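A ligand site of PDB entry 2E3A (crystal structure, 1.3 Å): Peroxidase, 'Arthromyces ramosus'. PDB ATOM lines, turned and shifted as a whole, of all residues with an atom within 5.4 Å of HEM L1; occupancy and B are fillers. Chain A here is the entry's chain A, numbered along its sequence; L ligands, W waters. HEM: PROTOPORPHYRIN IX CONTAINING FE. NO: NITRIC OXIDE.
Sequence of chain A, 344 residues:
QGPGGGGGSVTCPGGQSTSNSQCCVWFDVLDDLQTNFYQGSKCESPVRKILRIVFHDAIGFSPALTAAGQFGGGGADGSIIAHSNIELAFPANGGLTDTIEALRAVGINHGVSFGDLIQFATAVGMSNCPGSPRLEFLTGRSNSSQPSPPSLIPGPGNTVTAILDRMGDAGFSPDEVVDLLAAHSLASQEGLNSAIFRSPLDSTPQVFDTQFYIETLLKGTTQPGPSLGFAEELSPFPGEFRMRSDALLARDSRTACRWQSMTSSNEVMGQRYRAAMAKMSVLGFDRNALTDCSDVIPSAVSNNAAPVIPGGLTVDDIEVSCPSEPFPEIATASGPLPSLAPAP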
ATOM      1  N   SER A  45     -20.104  -1.695 -10.973  1.00  0.00           N
ATOM      2  CA  SER A  45     -19.792  -0.735 -11.980  1.00  0.00           C
ATOM      3  C   SER A  45     -18.412  -0.108 -11.802  1.00  0.00           C
ATOM      4  O   SER A  45     -17.754   0.002 -12.840  1.00  0.00           O
ATOM      5  CB  SER A  45     -20.904   0.315 -12.106  1.00  0.00           C
ATOM      6  OG  SER A  45     -20.634   1.180 -13.168  1.00  0.00           O
ATOM      7  N   VAL A  47     -15.446  -1.256 -10.929  1.00  0.00           N
ATOM      8  CA  VAL A  47     -14.453  -2.118 -11.555  1.00  0.00           C
ATOM      9  C   VAL A  47     -14.550  -2.037 -13.072  1.00  0.00           C
ATOM     10  O   VAL A  47     -13.558  -1.918 -13.812  1.00  0.00           O
ATOM     11  CB  VAL A  47     -14.532  -3.592 -11.065  1.00  0.00           C
ATOM     12  CG1 VAL A  47     -13.428  -4.385 -11.766  1.00  0.00           C
ATOM     13  CG2 VAL A  47     -14.392  -3.700  -9.581  1.00  0.00           C
ATOM     14  N   ARG A  48     -15.788  -2.114 -13.568  1.00  0.00           N
ATOM     15  CA  ARG A  48     -15.995  -2.159 -15.017  1.00  0.00           C
ATOM     16  C   ARG A  48     -15.558  -0.860 -15.683  1.00  0.00           C
ATOM     17  O   ARG A  48     -14.904  -0.889 -16.742  1.00  0.00           O
ATOM     18  CB  ARG A  48     -17.442  -2.544 -15.336  1.00  0.00           C
ATOM     19  CG  ARG A  48     -17.912  -3.785 -14.575  1.00  0.00           C
ATOM     20  CD  ARG A  48     -19.212  -4.348 -15.168  1.00  0.00           C
ATOM     21  NE  ARG A  48     -20.315  -3.417 -15.051  1.00  0.00           N
ATOM     22  CZ  ARG A  48     -21.231  -3.315 -14.107  1.00  0.00           C
ATOM     23  NH1 ARG A  48     -22.177  -2.396 -14.142  1.00  0.00           N
ATOM     24  NH2 ARG A  48     -21.202  -4.188 -13.082  1.00  0.00           N
ATOM     25  N   LYS A  49     -15.882   0.251 -15.048  1.00  0.00           N
ATOM     26  CA  LYS A  49     -15.448   1.532 -15.570  1.00  0.00           C
ATOM     27  C   LYS A  49     -13.929   1.657 -15.521  1.00  0.00           C
ATOM     28  O   LYS A  49     -13.318   2.188 -16.426  1.00  0.00           O
ATOM     29  CB  LYS A  49     -16.065   2.712 -14.771  1.00  0.00           C
ATOM     30  CG  LYS A  49     -17.578   2.797 -14.872  1.00  0.00           C
ATOM     31  CD  LYS A  49     -18.113   3.200 -16.217  1.00  0.00           C
ATOM     32  CE  LYS A  49     -19.619   3.407 -16.220  1.00  0.00           C
ATOM     33  NZ  LYS A  49     -20.040   4.014 -17.504  1.00  0.00           N
ATOM     34  N   LEU A  51     -11.802  -0.726 -15.809  1.00  0.00           N
ATOM     35  CA  LEU A  51     -11.232  -1.555 -16.888  1.00  0.00           C
ATOM     36  C   LEU A  51     -11.320  -0.805 -18.212  1.00  0.00           C
ATOM     37  O   LEU A  51     -10.410  -0.819 -19.029  1.00  0.00           O
ATOM     38  CB  LEU A  51     -11.875  -2.916 -16.923  1.00  0.00           C
ATOM     39  CG  LEU A  51     -11.493  -3.850 -15.781  1.00  0.00           C
ATOM     40  CD1 LEU A  51     -12.421  -5.045 -15.757  1.00  0.00           C
ATOM     41  CD2 LEU A  51     -10.022  -4.213 -15.846  1.00  0.00           C
ATOM     42  N   ARG A  52     -12.408  -0.115 -18.534  1.00  0.00           N
ATOM     43  CA  ARG A  52     -12.433   0.770 -19.695  1.00  0.00           C
ATOM     44  C   ARG A  52     -11.319   1.807 -19.616  1.00  0.00           C
ATOM     45  O   ARG A  52     -10.622   2.071 -20.615  1.00  0.00           O
ATOM     46  CB  ARG A  52     -13.773   1.476 -19.865  1.00  0.00           C
ATOM     47  CG  ARG A  52     -14.902   0.577 -20.287  1.00  0.00           C
ATOM     48  CD  ARG A  52     -16.200   1.357 -20.499  1.00  0.00           C
ATOM     49  NE  ARG A  52     -16.065   2.377 -21.534  1.00  0.00           N
ATOM     50  CZ  ARG A  52     -16.782   3.492 -21.514  1.00  0.00           C
ATOM     51  NH1 ARG A  52     -17.669   3.755 -20.550  1.00  0.00           N
ATOM     52  NH2 ARG A  52     -16.579   4.361 -22.519  1.00  0.00           N
ATOM     53  N   VAL A  54      -8.401   1.715 -17.969  1.00  0.00           N
ATOM     54  CA  VAL A  54      -7.031   1.219 -18.081  1.00  0.00           C
ATOM     55  C   VAL A  54      -6.686   0.982 -19.541  1.00  0.00           C
ATOM     56  O   VAL A  54      -5.607   1.307 -20.014  1.00  0.00           O
ATOM     57  CB  VAL A  54      -6.784  -0.005 -17.184  1.00  0.00           C
ATOM     58  CG1 VAL A  54      -7.490  -1.259 -17.695  1.00  0.00           C
ATOM     59  CG2 VAL A  54      -5.299  -0.272 -16.989  1.00  0.00           C
ATOM     60  N   PHE A  55      -7.607   0.426 -20.282  1.00  0.00           N
ATOM     61  CA  PHE A  55      -7.439   0.207 -21.699  1.00  0.00           C
ATOM     62  C   PHE A  55      -7.323   1.543 -22.417  1.00  0.00           C
ATOM     63  O   PHE A  55      -6.413   1.763 -23.240  1.00  0.00           O
ATOM     64  CB  PHE A  55      -8.584  -0.625 -22.233  1.00  0.00           C
ATOM     65  CG  PHE A  55      -8.586  -0.884 -23.735  1.00  0.00           C
ATOM     66  CD1 PHE A  55      -7.423  -1.123 -24.455  1.00  0.00           C
ATOM     67  CD2 PHE A  55      -9.782  -0.862 -24.423  1.00  0.00           C
ATOM     68  CE1 PHE A  55      -7.441  -1.354 -25.812  1.00  0.00           C
ATOM     69  CE2 PHE A  55      -9.814  -1.100 -25.796  1.00  0.00           C
ATOM     70  CZ  PHE A  55      -8.643  -1.339 -26.505  1.00  0.00           C
ATOM     71  N   PRO A 154      -9.850   1.662 -30.385  1.00  0.00           N
ATOM     72  CA  PRO A 154     -10.751   0.884 -31.235  1.00  0.00           C
ATOM     73  C   PRO A 154     -12.216   1.079 -30.835  1.00  0.00           C
ATOM     74  O   PRO A 154     -12.506   1.208 -29.661  1.00  0.00           O
ATOM     75  CB  PRO A 154     -10.305  -0.562 -30.976  1.00  0.00           C
ATOM     76  CG  PRO A 154      -8.887  -0.454 -30.561  1.00  0.00           C
ATOM     77  CD  PRO A 154      -8.810   0.810 -29.751  1.00  0.00           C
ATOM     78  N   GLY A 155     -13.066   1.146 -31.843  1.00  0.00           N
ATOM     79  CA  GLY A 155     -14.501   1.359 -31.661  1.00  0.00           C
ATOM     80  C   GLY A 155     -15.299   0.124 -32.068  1.00  0.00           C
ATOM     81  O   GLY A 155     -14.848  -0.726 -32.820  1.00  0.00           O
ATOM     82  N   PRO A 156     -16.496  -0.008 -31.501  1.00  0.00           N
ATOM     83  CA  PRO A 156     -17.268  -1.236 -31.672  1.00  0.00           C
ATOM     84  C   PRO A 156     -17.872  -1.418 -33.061  1.00  0.00           C
ATOM     85  O   PRO A 156     -18.264  -2.551 -33.375  1.00  0.00           O
ATOM     86  CB  PRO A 156     -18.400  -1.076 -30.656  1.00  0.00           C
ATOM     87  CG  PRO A 156     -18.526   0.399 -30.466  1.00  0.00           C
ATOM     88  CD  PRO A 156     -17.142   0.949 -30.614  1.00  0.00           C
ATOM     89  N   ILE A 163      -9.370  -2.992 -36.220  1.00  0.00           N
ATOM     90  CA  ILE A 163      -9.060  -3.233 -34.807  1.00  0.00           C
ATOM     91  C   ILE A 163      -7.702  -3.893 -34.669  1.00  0.00           C
ATOM     92  O   ILE A 163      -6.892  -3.488 -33.842  1.00  0.00           O
ATOM     93  CB  ILE A 163     -10.131  -4.120 -34.180  1.00  0.00           C
ATOM     94  CG1 ILE A 163     -11.471  -3.365 -34.166  1.00  0.00           C
ATOM     95  CG2 ILE A 163      -9.719  -4.642 -32.811  1.00  0.00           C
ATOM     96  CD1 ILE A 163     -12.621  -4.205 -33.666  1.00  0.00           C
ATOM     97  N   MET A 167      -4.559  -2.173 -32.781  1.00  0.00           N
ATOM     98  CA  MET A 167      -3.988  -2.917 -31.632  1.00  0.00           C
ATOM     99  C   MET A 167      -2.581  -3.347 -31.975  1.00  0.00           C
ATOM    100  O   MET A 167      -1.704  -3.364 -31.102  1.00  0.00           O
ATOM    101  CB  MET A 167      -4.865  -4.088 -31.258  1.00  0.00           C
ATOM    102  CG  MET A 167      -6.227  -3.730 -30.683  1.00  0.00           C
ATOM    103  SD  MET A 167      -6.189  -2.810 -29.133  1.00  0.00           S
ATOM    104  CE  MET A 167      -5.879  -4.154 -27.956  1.00  0.00           C
ATOM    105  N   VAL A 177      -5.140  -9.555 -28.585  1.00  0.00           N
ATOM    106  CA  VAL A 177      -6.403  -8.785 -28.628  1.00  0.00           C
ATOM    107  C   VAL A 177      -7.505  -9.627 -28.023  1.00  0.00           C
ATOM    108  O   VAL A 177      -8.253  -9.167 -27.166  1.00  0.00           O
ATOM    109  CB  VAL A 177      -6.724  -8.339 -30.055  1.00  0.00           C
ATOM    110  CG1 VAL A 177      -8.130  -7.733 -30.121  1.00  0.00           C
ATOM    111  CG2 VAL A 177      -5.669  -7.359 -30.575  1.00  0.00           C
ATOM    112  N   LEU A 180      -7.026  -9.904 -24.205  1.00  0.00           N
ATOM    113  CA  LEU A 180      -7.370  -8.686 -23.477  1.00  0.00           C
ATOM    114  C   LEU A 180      -8.903  -8.566 -23.334  1.00  0.00           C
ATOM    115  O   LEU A 180      -9.405  -8.029 -22.354  1.00  0.00           O
ATOM    116  CB  LEU A 180      -6.811  -7.450 -24.171  1.00  0.00           C
ATOM    117  CG  LEU A 180      -5.319  -7.178 -24.034  1.00  0.00           C
ATOM    118  CD1 LEU A 180      -4.916  -6.079 -25.015  1.00  0.00           C
ATOM    119  CD2 LEU A 180      -4.955  -6.810 -22.619  1.00  0.00           C
ATOM    120  N   LEU A 181      -9.628  -9.049 -24.338  1.00  0.00           N
ATOM    121  CA  LEU A 181     -11.078  -8.986 -24.353  1.00  0.00           C
ATOM    122  C   LEU A 181     -11.665  -9.884 -23.283  1.00  0.00           C
ATOM    123  O   LEU A 181     -12.866  -9.792 -23.096  1.00  0.00           O
ATOM    124  CB  LEU A 181     -11.623  -9.277 -25.741  1.00  0.00           C
ATOM    125  CG  LEU A 181     -11.679  -7.995 -26.595  1.00  0.00           C
ATOM    126  CD1 LEU A 181     -11.780  -8.375 -28.055  1.00  0.00           C
ATOM    127  CD2 LEU A 181     -12.884  -7.153 -26.224  1.00  0.00           C
ATOM    128  N   ALA A 183     -11.732  -9.098 -20.410  1.00  0.00           N
ATOM    129  CA  ALA A 183     -12.385  -8.105 -19.598  1.00  0.00           C
ATOM    130  C   ALA A 183     -13.866  -7.967 -19.926  1.00  0.00           C
ATOM    131  O   ALA A 183     -14.648  -7.570 -19.061  1.00  0.00           O
ATOM    132  CB  ALA A 183     -11.698  -6.750 -19.763  1.00  0.00           C
ATOM    133  N   HIS A 184     -14.296  -8.305 -21.117  1.00  0.00           N
ATOM    134  CA  HIS A 184     -15.730  -8.253 -21.460  1.00  0.00           C
ATOM    135  C   HIS A 184     -16.491  -9.351 -20.725  1.00  0.00           C
ATOM    136  O   HIS A 184     -17.731  -9.363 -20.825  1.00  0.00           O
ATOM    137  CB  HIS A 184     -15.959  -8.244 -22.965  1.00  0.00           C
ATOM    138  CG  HIS A 184     -15.727  -6.883 -23.585  1.00  0.00           C
ATOM    139  ND1 HIS A 184     -16.134  -6.562 -24.857  1.00  0.00           N
ATOM    140  CD2 HIS A 184     -15.102  -5.770 -23.145  1.00  0.00           C
ATOM    141  CE1 HIS A 184     -15.775  -5.297 -25.112  1.00  0.00           C
ATOM    142  NE2 HIS A 184     -15.139  -4.771 -24.078  1.00  0.00           N
ATOM    143  N   LEU A 186     -16.578  -9.125 -17.623  1.00  0.00           N
ATOM    144  CA  LEU A 186     -17.011  -8.331 -16.460  1.00  0.00           C
ATOM    145  C   LEU A 186     -17.568  -7.033 -17.012  1.00  0.00           C
ATOM    146  O   LEU A 186     -17.022  -5.972 -16.768  1.00  0.00           O
ATOM    147  CB  LEU A 186     -15.846  -8.020 -15.543  1.00  0.00           C
ATOM    148  CG  LEU A 186     -15.175  -9.197 -14.840  1.00  0.00           C
ATOM    149  CD1 LEU A 186     -13.869  -8.763 -14.171  1.00  0.00           C
ATOM    150  CD2 LEU A 186     -16.075  -9.887 -13.841  1.00  0.00           C
ATOM    151  N   ALA A 187     -18.673  -7.135 -17.758  1.00  0.00           N
ATOM    152  CA  ALA A 187     -18.994  -6.002 -18.605  1.00  0.00           C
ATOM    153  C   ALA A 187     -20.467  -5.827 -18.932  1.00  0.00           C
ATOM    154  O   ALA A 187     -21.260  -6.764 -18.977  1.00  0.00           O
ATOM    155  CB  ALA A 187     -18.231  -6.134 -19.920  1.00  0.00           C
ATOM    156  N   SER A 188     -20.830  -4.581 -19.177  1.00  0.00           N
ATOM    157  CA  SER A 188     -22.123  -4.124 -19.643  1.00  0.00           C
ATOM    158  C   SER A 188     -21.931  -2.946 -20.600  1.00  0.00           C
ATOM    159  O   SER A 188     -20.811  -2.436 -20.773  1.00  0.00           O
ATOM    160  CB  SER A 188     -23.026  -3.736 -18.467  1.00  0.00           C
ATOM    161  OG  SER A 188     -22.750  -2.454 -17.964  1.00  0.00           O
ATOM    162  N   GLN A 189     -23.030  -2.507 -21.219  1.00  0.00           N
ATOM    163  CA  GLN A 189     -22.986  -1.196 -21.848  1.00  0.00           C
ATOM    164  C   GLN A 189     -23.961  -0.224 -21.175  1.00  0.00           C
ATOM    165  O   GLN A 189     -25.071  -0.682 -20.843  1.00  0.00           O
ATOM    166  CB  GLN A 189     -23.261  -1.310 -23.351  1.00  0.00           C
ATOM    167  CG  GLN A 189     -24.647  -1.788 -23.774  1.00  0.00           C
ATOM    168  CD  GLN A 189     -25.706  -0.692 -23.808  1.00  0.00           C
ATOM    169  OE1 GLN A 189     -25.319   0.483 -24.064  1.00  0.00           O
ATOM    170  NE2 GLN A 189     -26.903  -1.086 -23.404  1.00  0.00           N
ATOM    171  N   GLU A 190     -23.605   1.039 -21.207  1.00  0.00           N
ATOM    172  CA  GLU A 190     -24.515   2.110 -20.848  1.00  0.00           C
ATOM    173  C   GLU A 190     -24.757   3.085 -21.964  1.00  0.00           C
ATOM    174  O   GLU A 190     -25.772   3.774 -21.961  1.00  0.00           O
ATOM    175  CB  GLU A 190     -23.966   2.909 -19.649  1.00  0.00           C
ATOM    176  CG  GLU A 190     -23.833   2.074 -18.420  1.00  0.00           C
ATOM    177  CD  GLU A 190     -23.199   2.727 -17.229  1.00  0.00           C
ATOM    178  OE1 GLU A 190     -22.866   3.935 -17.340  1.00  0.00           O
ATOM    179  OE2 GLU A 190     -23.002   2.092 -16.191  1.00  0.00           O
ATOM    180  N   GLY A 191     -23.832   3.217 -22.902  1.00  0.00           N
ATOM    181  CA  GLY A 191     -23.848   4.318 -23.834  1.00  0.00           C
ATOM    182  C   GLY A 191     -24.207   3.962 -25.253  1.00  0.00           C
ATOM    183  O   GLY A 191     -24.345   4.829 -26.101  1.00  0.00           O
ATOM    184  N   LEU A 192     -24.310   2.681 -25.559  1.00  0.00           N
ATOM    185  CA  LEU A 192     -24.638   2.218 -26.903  1.00  0.00           C
ATOM    186  C   LEU A 192     -26.139   2.197 -27.107  1.00  0.00           C
ATOM    187  O   LEU A 192     -26.579   2.586 -28.198  1.00  0.00           O
ATOM    188  CB  LEU A 192     -24.041   0.819 -27.154  1.00  0.00           C
ATOM    189  CG  LEU A 192     -22.515   0.773 -27.143  1.00  0.00           C
ATOM    190  CD1 LEU A 192     -22.019  -0.654 -27.301  1.00  0.00           C
ATOM    191  CD2 LEU A 192     -21.884   1.671 -28.210  1.00  0.00           C
ATOM    192  N   LEU A 201     -22.657  -8.024 -21.159  1.00  0.00           N
ATOM    193  CA  LEU A 201     -22.060  -8.671 -22.332  1.00  0.00           C
ATOM    194  C   LEU A 201     -21.953 -10.175 -22.147  1.00  0.00           C
ATOM    195  O   LEU A 201     -21.812 -10.908 -23.138  1.00  0.00           O
ATOM    196  CB  LEU A 201     -20.729  -8.081 -22.698  1.00  0.00           C
ATOM    197  CG  LEU A 201     -20.617  -6.557 -22.826  1.00  0.00           C
ATOM    198  CD1 LEU A 201     -19.223  -6.156 -23.271  1.00  0.00           C
ATOM    199  CD2 LEU A 201     -21.718  -6.046 -23.753  1.00  0.00           C
ATOM    200  N   MET A 243     -22.077  -6.428 -28.971  1.00  0.00           N
ATOM    201  CA  MET A 243     -21.546  -5.358 -29.808  1.00  0.00           C
ATOM    202  C   MET A 243     -20.946  -6.013 -31.027  1.00  0.00           C
ATOM    203  O   MET A 243     -20.454  -7.160 -31.046  1.00  0.00           O
ATOM    204  CB  MET A 243     -20.559  -4.466 -29.068  1.00  0.00           C
ATOM    205  CG  MET A 243     -19.185  -5.035 -28.794  1.00  0.00           C
ATOM    206  SD  MET A 243     -18.149  -3.869 -27.893  1.00  0.00           S
ATOM    207  CE  MET A 243     -18.955  -4.048 -26.285  1.00  0.00           C
ATOM    208  N   SER A 245     -18.176  -5.508 -32.788  1.00  0.00           N
ATOM    209  CA  SER A 245     -16.782  -5.882 -32.779  1.00  0.00           C
ATOM    210  C   SER A 245     -16.598  -7.273 -32.150  1.00  0.00           C
ATOM    211  O   SER A 245     -15.838  -8.073 -32.710  1.00  0.00           O
ATOM    212  CB  SER A 245     -15.943  -4.797 -32.135  1.00  0.00           C
ATOM    213  OG  SER A 245     -16.460  -4.432 -30.884  1.00  0.00           O
ATOM    214  N   LEU A 249     -15.174 -10.505 -34.050  1.00  0.00           N
ATOM    215  CA  LEU A 249     -13.904 -11.084 -33.628  1.00  0.00           C
ATOM    216  C   LEU A 249     -14.086 -12.570 -33.307  1.00  0.00           C
ATOM    217  O   LEU A 249     -13.216 -13.388 -33.552  1.00  0.00           O
ATOM    218  CB  LEU A 249     -13.403 -10.294 -32.411  1.00  0.00           C
ATOM    219  CG  LEU A 249     -12.768  -8.939 -32.722  1.00  0.00           C
ATOM    220  CD1 LEU A 249     -12.628  -8.077 -31.493  1.00  0.00           C
ATOM    221  CD2 LEU A 249     -11.396  -9.184 -33.377  1.00  0.00           C
ATOM    222  N   TYR A 273      -4.874 -13.504 -19.933  1.00  0.00           N
ATOM    223  CA  TYR A 273      -5.274 -12.134 -19.633  1.00  0.00           C
ATOM    224  C   TYR A 273      -4.232 -11.456 -18.754  1.00  0.00           C
ATOM    225  O   TYR A 273      -3.841 -10.289 -18.978  1.00  0.00           O
ATOM    226  CB  TYR A 273      -6.588 -12.148 -18.929  1.00  0.00           C
ATOM    227  CG  TYR A 273      -7.166 -10.869 -18.478  1.00  0.00           C
ATOM    228  CD1 TYR A 273      -7.721  -9.955 -19.332  1.00  0.00           C
ATOM    229  CD2 TYR A 273      -7.207 -10.539 -17.131  1.00  0.00           C
ATOM    230  CE1 TYR A 273      -8.279  -8.756 -18.939  1.00  0.00           C
ATOM    231  CE2 TYR A 273      -7.782  -9.350 -16.715  1.00  0.00           C
ATOM    232  CZ  TYR A 273      -8.313  -8.441 -17.606  1.00  0.00           C
ATOM    233  OH  TYR A 273      -8.912  -7.269 -17.172  1.00  0.00           O
ATOM    234  N   MET A 277      -2.380  -8.047 -19.911  1.00  0.00           N
ATOM    235  CA  MET A 277      -2.535  -6.863 -19.086  1.00  0.00           C
ATOM    236  C   MET A 277      -1.183  -6.332 -18.585  1.00  0.00           C
ATOM    237  O   MET A 277      -1.005  -5.109 -18.581  1.00  0.00           O
ATOM    238  CB  MET A 277      -3.505  -7.171 -17.953  1.00  0.00           C
ATOM    239  CG  MET A 277      -4.955  -7.381 -18.325  1.00  0.00           C
ATOM    240  SD  MET A 277      -5.721  -5.911 -19.042  1.00  0.00           S
ATOM    241  CE  MET A 277      -6.023  -5.006 -17.529  1.00  0.00           C
ATOM    242  N   MET A 280       0.232  -4.471 -21.505  1.00  0.00           N
ATOM    243  CA  MET A 280      -0.474  -3.217 -21.716  1.00  0.00           C
ATOM    244  C   MET A 280      -0.113  -2.186 -20.663  1.00  0.00           C
ATOM    245  O   MET A 280      -0.046  -0.960 -20.946  1.00  0.00           O
ATOM    246  CB  MET A 280      -1.991  -3.473 -21.729  1.00  0.00           C
ATOM    247  CG  MET A 280      -2.755  -2.249 -22.108  1.00  0.00           C
ATOM    248  SD  MET A 280      -4.497  -2.538 -22.437  1.00  0.00           S
ATOM    249  CE  MET A 280      -5.097  -2.648 -20.755  1.00  0.00           C
HETATM  250  CHA HEM L   1     -17.359  -1.980 -22.353  1.00  0.00           C
HETATM  251  CHB HEM L   1     -15.692  -1.682 -26.895  1.00  0.00           C
HETATM  252  CHC HEM L   1     -11.664  -3.911 -25.489  1.00  0.00           C
HETATM  253  CHD HEM L   1     -13.017  -3.457 -20.876  1.00  0.00           C
HETATM  254  C1A HEM L   1     -17.277  -1.687 -23.724  1.00  0.00           C
HETATM  255  C2A HEM L   1     -18.196  -0.862 -24.474  1.00  0.00           C
HETATM  256  C3A HEM L   1     -17.681  -0.720 -25.715  1.00  0.00           C
HETATM  257  C4A HEM L   1     -16.442  -1.481 -25.750  1.00  0.00           C
HETATM  258  CMA HEM L   1     -18.294  -0.012 -26.911  1.00  0.00           C
HETATM  259  CAA HEM L   1     -19.479  -0.337 -23.873  1.00  0.00           C
HETATM  260  CBA HEM L   1     -19.276   0.960 -23.104  1.00  0.00           C
HETATM  261  CGA HEM L   1     -20.621   1.567 -22.749  1.00  0.00           C
HETATM  262  O1A HEM L   1     -20.918   1.769 -21.553  1.00  0.00           O
HETATM  263  O2A HEM L   1     -21.400   1.880 -23.638  1.00  0.00           O
HETATM  264  C1B HEM L   1     -14.465  -2.322 -26.933  1.00  0.00           C
HETATM  265  C2B HEM L   1     -13.699  -2.576 -28.124  1.00  0.00           C
HETATM  266  C3B HEM L   1     -12.603  -3.348 -27.780  1.00  0.00           C
HETATM  267  C4B HEM L   1     -12.680  -3.408 -26.311  1.00  0.00           C
HETATM  268  CMB HEM L   1     -14.172  -2.184 -29.507  1.00  0.00           C
HETATM  269  CAB HEM L   1     -11.533  -3.741 -28.631  1.00  0.00           C
HETATM  270  CBB HEM L   1     -11.564  -4.652 -29.728  1.00  0.00           C
HETATM  271  C1C HEM L   1     -11.626  -3.889 -24.099  1.00  0.00           C
HETATM  272  C2C HEM L   1     -10.443  -4.133 -23.300  1.00  0.00           C
HETATM  273  C3C HEM L   1     -10.790  -3.937 -21.978  1.00  0.00           C
HETATM  274  C4C HEM L   1     -12.226  -3.595 -22.018  1.00  0.00           C
HETATM  275  CMC HEM L   1      -9.076  -4.488 -23.834  1.00  0.00           C
HETATM  276  CAC HEM L   1     -10.027  -3.920 -20.801  1.00  0.00           C
HETATM  277  CBC HEM L   1      -8.943  -4.821 -20.534  1.00  0.00           C
HETATM  278  C1D HEM L   1     -14.397  -3.253 -20.912  1.00  0.00           C
HETATM  279  C2D HEM L   1     -15.308  -3.335 -19.791  1.00  0.00           C
HETATM  280  C3D HEM L   1     -16.498  -2.856 -20.210  1.00  0.00           C
HETATM  281  C4D HEM L   1     -16.381  -2.553 -21.581  1.00  0.00           C
HETATM  282  CMD HEM L   1     -14.952  -3.819 -18.417  1.00  0.00           C
HETATM  283  CAD HEM L   1     -17.750  -2.782 -19.342  1.00  0.00           C
HETATM  284  CBD HEM L   1     -18.063  -1.349 -18.826  1.00  0.00           C
HETATM  285  CGD HEM L   1     -19.301  -1.278 -17.977  1.00  0.00           C
HETATM  286  O1D HEM L   1     -19.591  -0.130 -17.570  1.00  0.00           O
HETATM  287  O2D HEM L   1     -19.891  -2.314 -17.625  1.00  0.00           O
HETATM  288  NA  HEM L   1     -16.145  -1.991 -24.490  1.00  0.00           N
HETATM  289  NB  HEM L   1     -13.828  -2.809 -25.812  1.00  0.00           N
HETATM  290  NC  HEM L   1     -12.715  -3.506 -23.304  1.00  0.00           N
HETATM  291  ND  HEM L   1     -15.103  -2.835 -22.033  1.00  0.00           N
HETATM  292 FE   HEM L   1     -14.447  -2.812 -23.905  1.00  0.00          FE
HETATM  293  N    NO L   2     -13.710  -1.015 -23.745  1.00  0.00           N
HETATM  294  O    NO L   2     -12.953  -0.652 -22.861  1.00  0.00           O
HETATM  295  O   HOH W   1     -14.734  -5.607 -29.177  1.00  0.00           O
HETATM  296  O   HOH W   2     -21.298   0.011 -15.554  1.00  0.00           O
HETATM  297  O   HOH W   3     -20.334   3.561 -25.493  1.00  0.00           O
HETATM  298  O   HOH W   4     -19.448   1.941 -19.256  1.00  0.00           O
HETATM  299  O   HOH W   5     -14.374   1.246 -27.743  1.00  0.00           O
HETATM  300  O   HOH W   6     -20.663   4.624 -21.080  1.00  0.00           O
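Merely in contact with HEM L1: Phe 55 (3.4 Å), Leu 186 (3.4 Å), Ala 187 (3.4 Å), Met 243 (3.4 Å), Ala 183 (3.4 Å), Ser 245 (3.5 Å), Leu 51 (3.5 Å), Leu 181 (3.5 Å), Leu 192 (3.6 Å), Pro 156 (3.6 Å), Ile 163 (3.6 Å), Gln 189 (3.6 Å), Gly 155 (3.6 Å), Met 277 (3.7 Å), Leu 180 (3.7 Å), Pro 154 (3.8 Å), Lys 49 (3.8 Å) and Leu 249 (3.997 Å). Hydrophobic or aromatic side chains within 4 Å of HEM L1: Leu 51, Phe 55, Pro 156, Ile 163, Leu 180, Leu 181, Ala 183, His 184, Ala 187, Leu 192, Met 243, Leu 249 and Met 277.
The side-chain sulfur of Met 243 sits at hydrogen-bond distance from the side-chain hydroxyl of Ser 245 (3.5 Å). The backbone NH (N) of Leu 201 lies within hydrogen-bond range of the backbone carbonyl oxygen (O) of Ala 187, 2.9 Å away. The side-chain carboxylate of Glu 190 lies within salt-bridge range of the side-chain amino group of Lys 49 (2.8 Å). N of Gly 191 is in hydrogen-bond range of OE1 of Gln 189. The backbone carbonyl oxygen of Pro 156 sits at hydrogen-bond distance from the backbone NH of Ser 245 (3.0 Å). The side-chain amide oxygen (OE1) of Gln 189 is in hydrogen-bond range of the backbone NH (N) of Leu 192 (2.8 Å).
Water W2 lies within hydrogen-bond range of an oxygen (O1D) of HEM L1 (2.6 Å), the side-chain hydroxyl of Ser 45 (2.7 Å), the side-chain carboxylate of Glu 190 (2.8 Å) and the guanidinium group of Arg 48 (2.9 Å). Water W4 lies within hydrogen-bond range of O1D of HEM L1 (2.7 Å), NZ of Lys 49 (2.8 Å) and NH1 of Arg 52 (2.9 Å). Water W6 bridges O1A of HEM L1 (2.9 Å) and NH1 of Arg 52 (3.2 Å).
An oxygen (O2A) of HEM L1 sits at hydrogen-bond distance from the backbone NH of Gly 191, 2.9 Å away. The guanidinium group (NE) of Arg 48 is in salt-bridge range of an oxygen (O2D) of HEM L1 (2.8 Å). The backbone NH of Ser 188 sits at hydrogen-bond distance from an oxygen (O2D) of HEM L1, 2.9 Å away. An oxygen (O2D) of HEM L1 is in hydrogen-bond range of the side-chain hydroxyl (OG) of Ser 188. An iron atom (FE) of HEM L1 is bound by a ring nitrogen (NE2) of His 184 (2.1 Å). The backbone NH (N) of Glu 190 is in hydrogen-bond range of an oxygen (O1A) of HEM L1. O1A of HEM L1 is in salt-bridge range of NH1 of Arg 52, at 3.9 Å.
N of NO L2 is bound to FE of HEM L1 (1.9 Å).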
